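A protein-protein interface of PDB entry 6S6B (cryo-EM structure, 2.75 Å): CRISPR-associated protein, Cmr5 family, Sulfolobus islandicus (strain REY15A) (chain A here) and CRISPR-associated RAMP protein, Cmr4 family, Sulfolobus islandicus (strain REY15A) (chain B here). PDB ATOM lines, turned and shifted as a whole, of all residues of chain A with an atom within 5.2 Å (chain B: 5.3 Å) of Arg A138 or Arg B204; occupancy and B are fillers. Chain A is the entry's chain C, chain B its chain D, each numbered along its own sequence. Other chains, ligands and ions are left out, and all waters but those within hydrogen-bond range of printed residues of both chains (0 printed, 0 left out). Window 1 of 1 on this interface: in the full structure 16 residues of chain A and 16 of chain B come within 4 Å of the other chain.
The side-chain hydroxyl (OH) of Tyr A42 is in hydrogen-bond range of the backbone carbonyl oxygen (O) of Asn B203 (3.1 Å). The backbone carbonyl oxygen (O) of Tyr A42 is in hydrogen-bond range of the guanidinium group (NH2) of Arg B204, 2.8 Å away. The side-chain hydroxyl (OH) of Tyr A42 lies close to the backbone NH (N) of Leu B206, 3.2 Å away. The side-chain hydroxyl of Ser A134 sits at hydrogen-bond distance from the side-chain carboxylate of Glu B200, 3.0 Å away. The backbone NH (N) of Ala A135 sits at hydrogen-bond distance from the side-chain carboxylate (OE1) of Glu B200, at 2.9 Å. The backbone NH (N) of Gly A45 sits close to the guanidinium group (NH2) of Arg B204, at 2.9 Å.
OG of Ser A134 is in hydrogen-bond range of NH2 of Arg A138 (2.9 Å). The side-chain carboxylate of Glu B29 lies within salt-bridge range of the guanidinium group of Arg B208 (3.7 Å). The backbone carbonyl oxygen (O) of Arg B204 sits at hydrogen-bond distance from the guanidinium group (NH2) of Arg B97 (3.0 Å). The side-chain carboxylate (OE1) of Glu B167 is in salt-bridge range of the guanidinium group (NH2) of Arg B204, at 3.0 Å.
Among the printed residues, pairs that only touch across the chains: Ile A41 with Arg B204, Tyr A42 with Arg B208, Asn A43 with Arg B204, Asn A43 with Arg B208, Ser A44 with Arg B204, Gly A45 with Asp B168, Ser A134 with Phe B169, Arg A138 with Glu B29, Arg A138 with Arg B204 and Leu A142 with Glu B29.
Hydrophobic or aromatic side chains of chain B that line the printed part of chain A: Phe B169 and Leu B206. Hydrophobic or aromatic side chains of chain A that line the printed part of chain B: Tyr A42, Ala A135 and Leu A142. Among the printed residues, 16 pairs touch across the chains.
Of the printed residues of chain B, Ala A135 touches Glu B200. Of the printed residues of chain B, Arg A138 touches Glu B29 and Arg B204. Leu B165 touches none of the printed residues of chain A. Of the printed residues of chain A, Glu B200 touches Ser A134 (3.0 Å) and Ala A135 (2.9 Å). Printed residues of chain A within 4 Å of Asn B203: Tyr A42. The nearest residue of chain B that does not touch Arg A138 is Arg B208 (5.0 Å).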
ATOM      1  N   VAL A  38      -9.569 -13.191  21.736  1.00  0.00           N
ATOM      2  CA  VAL A  38      -8.879 -11.915  21.856  1.00  0.00           C
ATOM      3  C   VAL A  38      -7.391 -12.133  22.084  1.00  0.00           C
ATOM      4  O   VAL A  38      -6.574 -11.277  21.737  1.00  0.00           O
ATOM      5  CB  VAL A  38      -9.510 -11.068  22.976  1.00  0.00           C
ATOM      6  CG1 VAL A  38      -9.192 -11.651  24.341  1.00  0.00           C
ATOM      7  CG2 VAL A  38      -9.042  -9.631  22.884  1.00  0.00           C
ATOM      8  N   ILE A  41      -5.940 -13.068  18.440  1.00  0.00           N
ATOM      9  CA  ILE A  41      -5.757 -11.953  17.524  1.00  0.00           C
ATOM     10  C   ILE A  41      -4.397 -11.309  17.726  1.00  0.00           C
ATOM     11  O   ILE A  41      -3.784 -10.821  16.772  1.00  0.00           O
ATOM     12  CB  ILE A  41      -6.907 -10.949  17.701  1.00  0.00           C
ATOM     13  CG1 ILE A  41      -8.179 -11.522  17.087  1.00  0.00           C
ATOM     14  CG2 ILE A  41      -6.568  -9.617  17.081  1.00  0.00           C
ATOM     15  CD1 ILE A  41      -9.277 -10.531  16.936  1.00  0.00           C
ATOM     16  N   TYR A  42      -3.886 -11.314  18.952  1.00  0.00           N
ATOM     17  CA  TYR A  42      -2.551 -10.776  19.170  1.00  0.00           C
ATOM     18  C   TYR A  42      -1.486 -11.726  18.652  1.00  0.00           C
ATOM     19  O   TYR A  42      -0.514 -11.295  18.023  1.00  0.00           O
ATOM     20  CB  TYR A  42      -2.325 -10.489  20.651  1.00  0.00           C
ATOM     21  CG  TYR A  42      -0.906 -10.081  20.960  1.00  0.00           C
ATOM     22  CD1 TYR A  42       0.061 -11.025  21.243  1.00  0.00           C
ATOM     23  CD2 TYR A  42      -0.532  -8.749  20.958  1.00  0.00           C
ATOM     24  CE1 TYR A  42       1.352 -10.661  21.511  1.00  0.00           C
ATOM     25  CE2 TYR A  42       0.760  -8.374  21.234  1.00  0.00           C
ATOM     26  CZ  TYR A  42       1.697  -9.337  21.509  1.00  0.00           C
ATOM     27  OH  TYR A  42       2.993  -8.983  21.787  1.00  0.00           O
ATOM     28  N   ASN A  43      -1.639 -13.020  18.913  1.00  0.00           N
ATOM     29  CA  ASN A  43      -0.567 -13.956  18.615  1.00  0.00           C
ATOM     30  C   ASN A  43      -0.462 -14.260  17.133  1.00  0.00           C
ATOM     31  O   ASN A  43       0.635 -14.533  16.643  1.00  0.00           O
ATOM     32  CB  ASN A  43      -0.771 -15.245  19.401  1.00  0.00           C
ATOM     33  CG  ASN A  43      -0.352 -15.112  20.842  1.00  0.00           C
ATOM     34  OD1 ASN A  43      -1.165 -15.249  21.751  1.00  0.00           O
ATOM     35  ND2 ASN A  43       0.926 -14.842  21.061  1.00  0.00           N
ATOM     36  N   SER A  44      -1.574 -14.208  16.401  1.00  0.00           N
ATOM     37  CA  SER A  44      -1.565 -14.531  14.980  1.00  0.00           C
ATOM     38  C   SER A  44      -2.158 -13.416  14.132  1.00  0.00           C
ATOM     39  O   SER A  44      -2.631 -13.674  13.027  1.00  0.00           O
ATOM     40  CB  SER A  44      -2.317 -15.835  14.720  1.00  0.00           C
ATOM     41  OG  SER A  44      -3.640 -15.752  15.208  1.00  0.00           O
ATOM     42  N   GLY A  45      -2.153 -12.187  14.623  1.00  0.00           N
ATOM     43  CA  GLY A  45      -2.627 -11.075  13.828  1.00  0.00           C
ATOM     44  C   GLY A  45      -4.131 -11.038  13.699  1.00  0.00           C
ATOM     45  O   GLY A  45      -4.810 -12.025  13.986  1.00  0.00           O
ATOM     46  N   ILE A 133      -7.197  -1.024  12.174  1.00  0.00           N
ATOM     47  CA  ILE A 133      -7.931  -1.978  12.995  1.00  0.00           C
ATOM     48  C   ILE A 133      -7.125  -2.354  14.227  1.00  0.00           C
ATOM     49  O   ILE A 133      -7.643  -2.372  15.349  1.00  0.00           O
ATOM     50  CB  ILE A 133      -8.296  -3.224  12.171  1.00  0.00           C
ATOM     51  CG1 ILE A 133      -9.304  -2.876  11.081  1.00  0.00           C
ATOM     52  CG2 ILE A 133      -8.848  -4.299  13.066  1.00  0.00           C
ATOM     53  CD1 ILE A 133      -9.239  -3.800   9.899  1.00  0.00           C
ATOM     54  N   SER A 134      -5.840  -2.650  14.041  1.00  0.00           N
ATOM     55  CA  SER A 134      -5.047  -3.233  15.117  1.00  0.00           C
ATOM     56  C   SER A 134      -4.915  -2.284  16.300  1.00  0.00           C
ATOM     57  O   SER A 134      -4.976  -2.707  17.459  1.00  0.00           O
ATOM     58  CB  SER A 134      -3.669  -3.630  14.595  1.00  0.00           C
ATOM     59  OG  SER A 134      -2.768  -3.821  15.668  1.00  0.00           O
ATOM     60  N   ALA A 135      -4.713  -0.997  16.025  1.00  0.00           N
ATOM     61  CA  ALA A 135      -4.553  -0.021  17.096  1.00  0.00           C
ATOM     62  C   ALA A 135      -5.735  -0.047  18.054  1.00  0.00           C
ATOM     63  O   ALA A 135      -5.563  -0.017  19.276  1.00  0.00           O
ATOM     64  CB  ALA A 135      -4.380   1.376  16.504  1.00  0.00           C
ATOM     65  N   LYS A 136      -6.944  -0.116  17.512  1.00  0.00           N
ATOM     66  CA  LYS A 136      -8.141   0.076  18.315  1.00  0.00           C
ATOM     67  C   LYS A 136      -8.769  -1.229  18.790  1.00  0.00           C
ATOM     68  O   LYS A 136      -8.966  -1.417  19.992  1.00  0.00           O
ATOM     69  CB  LYS A 136      -9.162   0.880  17.518  1.00  0.00           C
ATOM     70  CG  LYS A 136      -9.148   2.368  17.812  1.00  0.00           C
ATOM     71  CD  LYS A 136     -10.196   3.101  16.988  1.00  0.00           C
ATOM     72  CE  LYS A 136      -9.822   3.136  15.517  1.00  0.00           C
ATOM     73  NZ  LYS A 136     -10.709   4.047  14.751  1.00  0.00           N
ATOM     74  N   ILE A 137      -9.077  -2.132  17.860  1.00  0.00           N
ATOM     75  CA  ILE A 137     -10.004  -3.237  18.090  1.00  0.00           C
ATOM     76  C   ILE A 137      -9.671  -4.046  19.335  1.00  0.00           C
ATOM     77  O   ILE A 137     -10.569  -4.592  19.981  1.00  0.00           O
ATOM     78  CB  ILE A 137     -10.070  -4.159  16.860  1.00  0.00           C
ATOM     79  CG1 ILE A 137     -11.294  -5.063  16.947  1.00  0.00           C
ATOM     80  CG2 ILE A 137      -8.818  -4.996  16.738  1.00  0.00           C
ATOM     81  CD1 ILE A 137     -11.643  -5.732  15.654  1.00  0.00           C
ATOM     82  N   ARG A 138      -8.395  -4.120  19.698  1.00  0.00           N
ATOM     83  CA  ARG A 138      -8.028  -5.046  20.759  1.00  0.00           C
ATOM     84  C   ARG A 138      -8.410  -4.552  22.144  1.00  0.00           C
ATOM     85  O   ARG A 138      -8.171  -5.268  23.117  1.00  0.00           O
ATOM     86  CB  ARG A 138      -6.531  -5.342  20.704  1.00  0.00           C
ATOM     87  CG  ARG A 138      -6.189  -6.785  21.014  1.00  0.00           C
ATOM     88  CD  ARG A 138      -4.714  -7.064  20.830  1.00  0.00           C
ATOM     89  NE  ARG A 138      -4.302  -6.863  19.449  1.00  0.00           N
ATOM     90  CZ  ARG A 138      -3.430  -5.944  19.055  1.00  0.00           C
ATOM     91  NH1 ARG A 138      -2.869  -5.134  19.942  1.00  0.00           N
ATOM     92  NH2 ARG A 138      -3.120  -5.835  17.772  1.00  0.00           N
ATOM     93  N   THR A 139      -8.992  -3.363  22.264  1.00  0.00           N
ATOM     94  CA  THR A 139      -9.558  -2.915  23.528  1.00  0.00           C
ATOM     95  C   THR A 139     -11.075  -2.880  23.517  1.00  0.00           C
ATOM     96  O   THR A 139     -11.690  -2.859  24.582  1.00  0.00           O
ATOM     97  CB  THR A 139      -9.027  -1.527  23.897  1.00  0.00           C
ATOM     98  OG1 THR A 139      -9.449  -1.193  25.224  1.00  0.00           O
ATOM     99  CG2 THR A 139      -9.550  -0.491  22.943  1.00  0.00           C
ATOM    100  N   TYR A 140     -11.685  -2.867  22.336  1.00  0.00           N
ATOM    101  CA  TYR A 140     -13.115  -3.114  22.234  1.00  0.00           C
ATOM    102  C   TYR A 140     -13.420  -4.586  22.461  1.00  0.00           C
ATOM    103  O   TYR A 140     -14.447  -4.930  23.052  1.00  0.00           O
ATOM    104  CB  TYR A 140     -13.611  -2.656  20.868  1.00  0.00           C
ATOM    105  CG  TYR A 140     -14.827  -3.372  20.340  1.00  0.00           C
ATOM    106  CD1 TYR A 140     -16.095  -2.998  20.726  1.00  0.00           C
ATOM    107  CD2 TYR A 140     -14.702  -4.405  19.433  1.00  0.00           C
ATOM    108  CE1 TYR A 140     -17.200  -3.634  20.234  1.00  0.00           C
ATOM    109  CE2 TYR A 140     -15.803  -5.051  18.940  1.00  0.00           C
ATOM    110  CZ  TYR A 140     -17.048  -4.659  19.342  1.00  0.00           C
ATOM    111  OH  TYR A 140     -18.153  -5.299  18.850  1.00  0.00           O
ATOM    112  N   LEU A 141     -12.538  -5.468  21.997  1.00  0.00           N
ATOM    113  CA  LEU A 141     -12.737  -6.893  22.219  1.00  0.00           C
ATOM    114  C   LEU A 141     -12.442  -7.273  23.655  1.00  0.00           C
ATOM    115  O   LEU A 141     -12.984  -8.261  24.157  1.00  0.00           O
ATOM    116  CB  LEU A 141     -11.856  -7.701  21.277  1.00  0.00           C
ATOM    117  CG  LEU A 141     -12.160  -7.584  19.789  1.00  0.00           C
ATOM    118  CD1 LEU A 141     -11.219  -8.471  19.041  1.00  0.00           C
ATOM    119  CD2 LEU A 141     -13.591  -7.962  19.496  1.00  0.00           C
ATOM    120  N   LEU A 142     -11.581  -6.516  24.326  1.00  0.00           N
ATOM    121  CA  LEU A 142     -11.348  -6.755  25.742  1.00  0.00           C
ATOM    122  C   LEU A 142     -12.576  -6.408  26.568  1.00  0.00           C
ATOM    123  O   LEU A 142     -12.812  -7.016  27.614  1.00  0.00           O
ATOM    124  CB  LEU A 142     -10.141  -5.951  26.205  1.00  0.00           C
ATOM    125  CG  LEU A 142      -9.910  -5.881  27.703  1.00  0.00           C
ATOM    126  CD1 LEU A 142      -9.649  -7.273  28.231  1.00  0.00           C
ATOM    127  CD2 LEU A 142      -8.754  -4.960  28.000  1.00  0.00           C
ATOM    128  N   GLU B  29      -5.194  -6.786  28.554  1.00  0.00           N
ATOM    129  CA  GLU B  29      -5.682  -8.159  28.603  1.00  0.00           C
ATOM    130  C   GLU B  29      -4.555  -9.152  28.849  1.00  0.00           C
ATOM    131  O   GLU B  29      -4.710 -10.347  28.593  1.00  0.00           O
ATOM    132  CB  GLU B  29      -6.419  -8.501  27.310  1.00  0.00           C
ATOM    133  CG  GLU B  29      -5.532  -8.583  26.080  1.00  0.00           C
ATOM    134  CD  GLU B  29      -5.184  -7.224  25.493  1.00  0.00           C
ATOM    135  OE1 GLU B  29      -5.073  -6.243  26.258  1.00  0.00           O
ATOM    136  OE2 GLU B  29      -5.027  -7.136  24.259  1.00  0.00           O
ATOM    137  N   ARG B  97       9.162 -10.460  13.620  1.00  0.00           N
ATOM    138  CA  ARG B  97       9.244 -11.578  12.699  1.00  0.00           C
ATOM    139  C   ARG B  97       8.728 -11.164  11.331  1.00  0.00           C
ATOM    140  O   ARG B  97       7.741 -10.435  11.215  1.00  0.00           O
ATOM    141  CB  ARG B  97       8.472 -12.773  13.251  1.00  0.00           C
ATOM    142  CG  ARG B  97       6.981 -12.621  13.266  1.00  0.00           C
ATOM    143  CD  ARG B  97       6.368 -13.560  14.274  1.00  0.00           C
ATOM    144  NE  ARG B  97       6.216 -12.923  15.574  1.00  0.00           N
ATOM    145  CZ  ARG B  97       5.112 -12.308  15.977  1.00  0.00           C
ATOM    146  NH1 ARG B  97       4.055 -12.246  15.184  1.00  0.00           N
ATOM    147  NH2 ARG B  97       5.065 -11.757  17.179  1.00  0.00           N
ATOM    148  N   LEU B 165       5.246  -7.715   8.098  1.00  0.00           N
ATOM    149  CA  LEU B 165       5.784  -7.740   9.448  1.00  0.00           C
ATOM    150  C   LEU B 165       4.716  -8.240  10.406  1.00  0.00           C
ATOM    151  O   LEU B 165       3.606  -7.707  10.430  1.00  0.00           O
ATOM    152  CB  LEU B 165       6.260  -6.356   9.879  1.00  0.00           C
ATOM    153  CG  LEU B 165       7.639  -5.912   9.406  1.00  0.00           C
ATOM    154  CD1 LEU B 165       8.673  -6.914   9.830  1.00  0.00           C
ATOM    155  CD2 LEU B 165       7.677  -5.711   7.920  1.00  0.00           C
ATOM    156  N   ASN B 166       5.061  -9.258  11.190  1.00  0.00           N
ATOM    157  CA  ASN B 166       4.174  -9.811  12.208  1.00  0.00           C
ATOM    158  C   ASN B 166       2.828 -10.211  11.612  1.00  0.00           C
ATOM    159  O   ASN B 166       1.763  -9.904  12.148  1.00  0.00           O
ATOM    160  CB  ASN B 166       3.992  -8.828  13.361  1.00  0.00           C
ATOM    161  CG  ASN B 166       5.245  -8.654  14.175  1.00  0.00           C
ATOM    162  OD1 ASN B 166       6.033  -9.578  14.322  1.00  0.00           O
ATOM    163  ND2 ASN B 166       5.437  -7.465  14.715  1.00  0.00           N
ATOM    164  N   GLU B 167       2.888 -10.867  10.454  1.00  0.00           N
ATOM    165  CA  GLU B 167       1.753 -11.557   9.849  1.00  0.00           C
ATOM    166  C   GLU B 167       0.650 -10.626   9.377  1.00  0.00           C
ATOM    167  O   GLU B 167      -0.312 -11.078   8.750  1.00  0.00           O
ATOM    168  CB  GLU B 167       1.135 -12.557  10.829  1.00  0.00           C
ATOM    169  CG  GLU B 167       2.048 -13.656  11.280  1.00  0.00           C
ATOM    170  CD  GLU B 167       2.645 -13.395  12.638  1.00  0.00           C
ATOM    171  OE1 GLU B 167       2.123 -12.527  13.362  1.00  0.00           O
ATOM    172  OE2 GLU B 167       3.641 -14.055  12.982  1.00  0.00           O
ATOM    173  N   ASP B 168       0.764  -9.335   9.654  1.00  0.00           N
ATOM    174  CA  ASP B 168      -0.407  -8.478   9.583  1.00  0.00           C
ATOM    175  C   ASP B 168      -0.185  -7.164   8.856  1.00  0.00           C
ATOM    176  O   ASP B 168      -1.159  -6.588   8.367  1.00  0.00           O
ATOM    177  CB  ASP B 168      -0.913  -8.190  11.005  1.00  0.00           C
ATOM    178  CG  ASP B 168      -2.371  -7.796  11.039  1.00  0.00           C
ATOM    179  OD1 ASP B 168      -2.997  -7.733   9.969  1.00  0.00           O
ATOM    180  OD2 ASP B 168      -2.897  -7.567  12.148  1.00  0.00           O
ATOM    181  N   PHE B 169       1.047  -6.682   8.741  1.00  0.00           N
ATOM    182  CA  PHE B 169       1.321  -5.362   8.188  1.00  0.00           C
ATOM    183  C   PHE B 169       2.242  -5.515   6.989  1.00  0.00           C
ATOM    184  O   PHE B 169       3.408  -5.886   7.139  1.00  0.00           O
ATOM    185  CB  PHE B 169       1.938  -4.457   9.250  1.00  0.00           C
ATOM    186  CG  PHE B 169       1.274  -4.574  10.582  1.00  0.00           C
ATOM    187  CD1 PHE B 169       0.126  -3.860  10.860  1.00  0.00           C
ATOM    188  CD2 PHE B 169       1.780  -5.415  11.550  1.00  0.00           C
ATOM    189  CE1 PHE B 169      -0.497  -3.978  12.074  1.00  0.00           C
ATOM    190  CE2 PHE B 169       1.160  -5.534  12.767  1.00  0.00           C
ATOM    191  CZ  PHE B 169       0.020  -4.813  13.029  1.00  0.00           C
ATOM    192  N   GLU B 200       2.123  -0.233  15.562  1.00  0.00           N
ATOM    193  CA  GLU B 200       1.417  -1.504  15.519  1.00  0.00           C
ATOM    194  C   GLU B 200       2.384  -2.671  15.423  1.00  0.00           C
ATOM    195  O   GLU B 200       2.189  -3.699  16.077  1.00  0.00           O
ATOM    196  CB  GLU B 200       0.459  -1.526  14.336  1.00  0.00           C
ATOM    197  CG  GLU B 200      -0.364  -0.284  14.209  1.00  0.00           C
ATOM    198  CD  GLU B 200      -1.201  -0.044  15.434  1.00  0.00           C
ATOM    199  OE1 GLU B 200      -1.857  -1.002  15.888  1.00  0.00           O
ATOM    200  OE2 GLU B 200      -1.194   1.091  15.952  1.00  0.00           O
ATOM    201  N   VAL B 201       3.429  -2.530  14.613  1.00  0.00           N
ATOM    202  CA  VAL B 201       4.366  -3.626  14.418  1.00  0.00           C
ATOM    203  C   VAL B 201       5.118  -3.922  15.704  1.00  0.00           C
ATOM    204  O   VAL B 201       5.286  -5.086  16.085  1.00  0.00           O
ATOM    205  CB  VAL B 201       5.327  -3.300  13.261  1.00  0.00           C
ATOM    206  CG1 VAL B 201       6.344  -4.401  13.099  1.00  0.00           C
ATOM    207  CG2 VAL B 201       4.551  -3.106  11.985  1.00  0.00           C
ATOM    208  N   ILE B 202       5.579  -2.883  16.397  1.00  0.00           N
ATOM    209  CA  ILE B 202       6.401  -3.107  17.580  1.00  0.00           C
ATOM    210  C   ILE B 202       5.584  -3.711  18.708  1.00  0.00           C
ATOM    211  O   ILE B 202       6.085  -4.553  19.460  1.00  0.00           O
ATOM    212  CB  ILE B 202       7.079  -1.798  18.011  1.00  0.00           C
ATOM    213  CG1 ILE B 202       8.224  -1.465  17.060  1.00  0.00           C
ATOM    214  CG2 ILE B 202       7.605  -1.902  19.418  1.00  0.00           C
ATOM    215  CD1 ILE B 202       8.907  -0.171  17.369  1.00  0.00           C
ATOM    216  N   ASN B 203       4.318  -3.323  18.840  1.00  0.00           N
ATOM    217  CA  ASN B 203       3.521  -3.831  19.948  1.00  0.00           C
ATOM    218  C   ASN B 203       3.191  -5.303  19.770  1.00  0.00           C
ATOM    219  O   ASN B 203       3.227  -6.071  20.735  1.00  0.00           O
ATOM    220  CB  ASN B 203       2.252  -3.008  20.100  1.00  0.00           C
ATOM    221  CG  ASN B 203       2.473  -1.773  20.929  1.00  0.00           C
ATOM    222  OD1 ASN B 203       3.295  -1.770  21.845  1.00  0.00           O
ATOM    223  ND2 ASN B 203       1.746  -0.709  20.616  1.00  0.00           N
ATOM    224  N   ARG B 204       2.868  -5.719  18.553  1.00  0.00           N
ATOM    225  CA  ARG B 204       2.619  -7.129  18.297  1.00  0.00           C
ATOM    226  C   ARG B 204       3.895  -7.948  18.225  1.00  0.00           C
ATOM    227  O   ARG B 204       3.824  -9.159  18.011  1.00  0.00           O
ATOM    228  CB  ARG B 204       1.823  -7.296  17.006  1.00  0.00           C
ATOM    229  CG  ARG B 204       0.380  -6.873  17.134  1.00  0.00           C
ATOM    230  CD  ARG B 204      -0.482  -7.587  16.129  1.00  0.00           C
ATOM    231  NE  ARG B 204      -0.261  -9.022  16.195  1.00  0.00           N
ATOM    232  CZ  ARG B 204       0.251  -9.741  15.206  1.00  0.00           C
ATOM    233  NH1 ARG B 204       0.583  -9.157  14.068  1.00  0.00           N
ATOM    234  NH2 ARG B 204       0.427 -11.043  15.354  1.00  0.00           N
ATOM    235  N   SER B 205       5.048  -7.326  18.408  1.00  0.00           N
ATOM    236  CA  SER B 205       6.324  -8.015  18.355  1.00  0.00           C
ATOM    237  C   SER B 205       6.746  -8.578  19.701  1.00  0.00           C
ATOM    238  O   SER B 205       7.787  -9.231  19.782  1.00  0.00           O
ATOM    239  CB  SER B 205       7.403  -7.068  17.836  1.00  0.00           C
ATOM    240  OG  SER B 205       8.679  -7.664  17.929  1.00  0.00           O
ATOM    241  N   LEU B 206       5.975  -8.342  20.754  1.00  0.00           N
ATOM    242  CA  LEU B 206       6.301  -8.863  22.071  1.00  0.00           C
ATOM    243  C   LEU B 206       5.750 -10.269  22.224  1.00  0.00           C
ATOM    244  O   LEU B 206       4.640 -10.567  21.780  1.00  0.00           O
ATOM    245  CB  LEU B 206       5.736  -7.971  23.173  1.00  0.00           C
ATOM    246  CG  LEU B 206       6.470  -6.668  23.448  1.00  0.00           C
ATOM    247  CD1 LEU B 206       5.894  -5.572  22.597  1.00  0.00           C
ATOM    248  CD2 LEU B 206       6.372  -6.315  24.903  1.00  0.00           C
ATOM    249  N   ARG B 208       4.018 -13.242  24.073  1.00  0.00           N
ATOM    250  CA  ARG B 208       2.904 -13.242  25.009  1.00  0.00           C
ATOM    251  C   ARG B 208       2.529 -14.689  25.291  1.00  0.00           C
ATOM    252  O   ARG B 208       2.020 -15.384  24.409  1.00  0.00           O
ATOM    253  CB  ARG B 208       1.735 -12.457  24.432  1.00  0.00           C
ATOM    254  CG  ARG B 208       0.418 -12.679  25.098  1.00  0.00           C
ATOM    255  CD  ARG B 208      -0.524 -11.573  24.688  1.00  0.00           C
ATOM    256  NE  ARG B 208       0.089 -10.261  24.869  1.00  0.00           N
ATOM    257  CZ  ARG B 208      -0.567  -9.113  24.754  1.00  0.00           C
ATOM    258  NH1 ARG B 208      -1.855  -9.110  24.453  1.00  0.00           N
ATOM    259  NH2 ARG B 208       0.067  -7.966  24.937  1.00  0.00           N
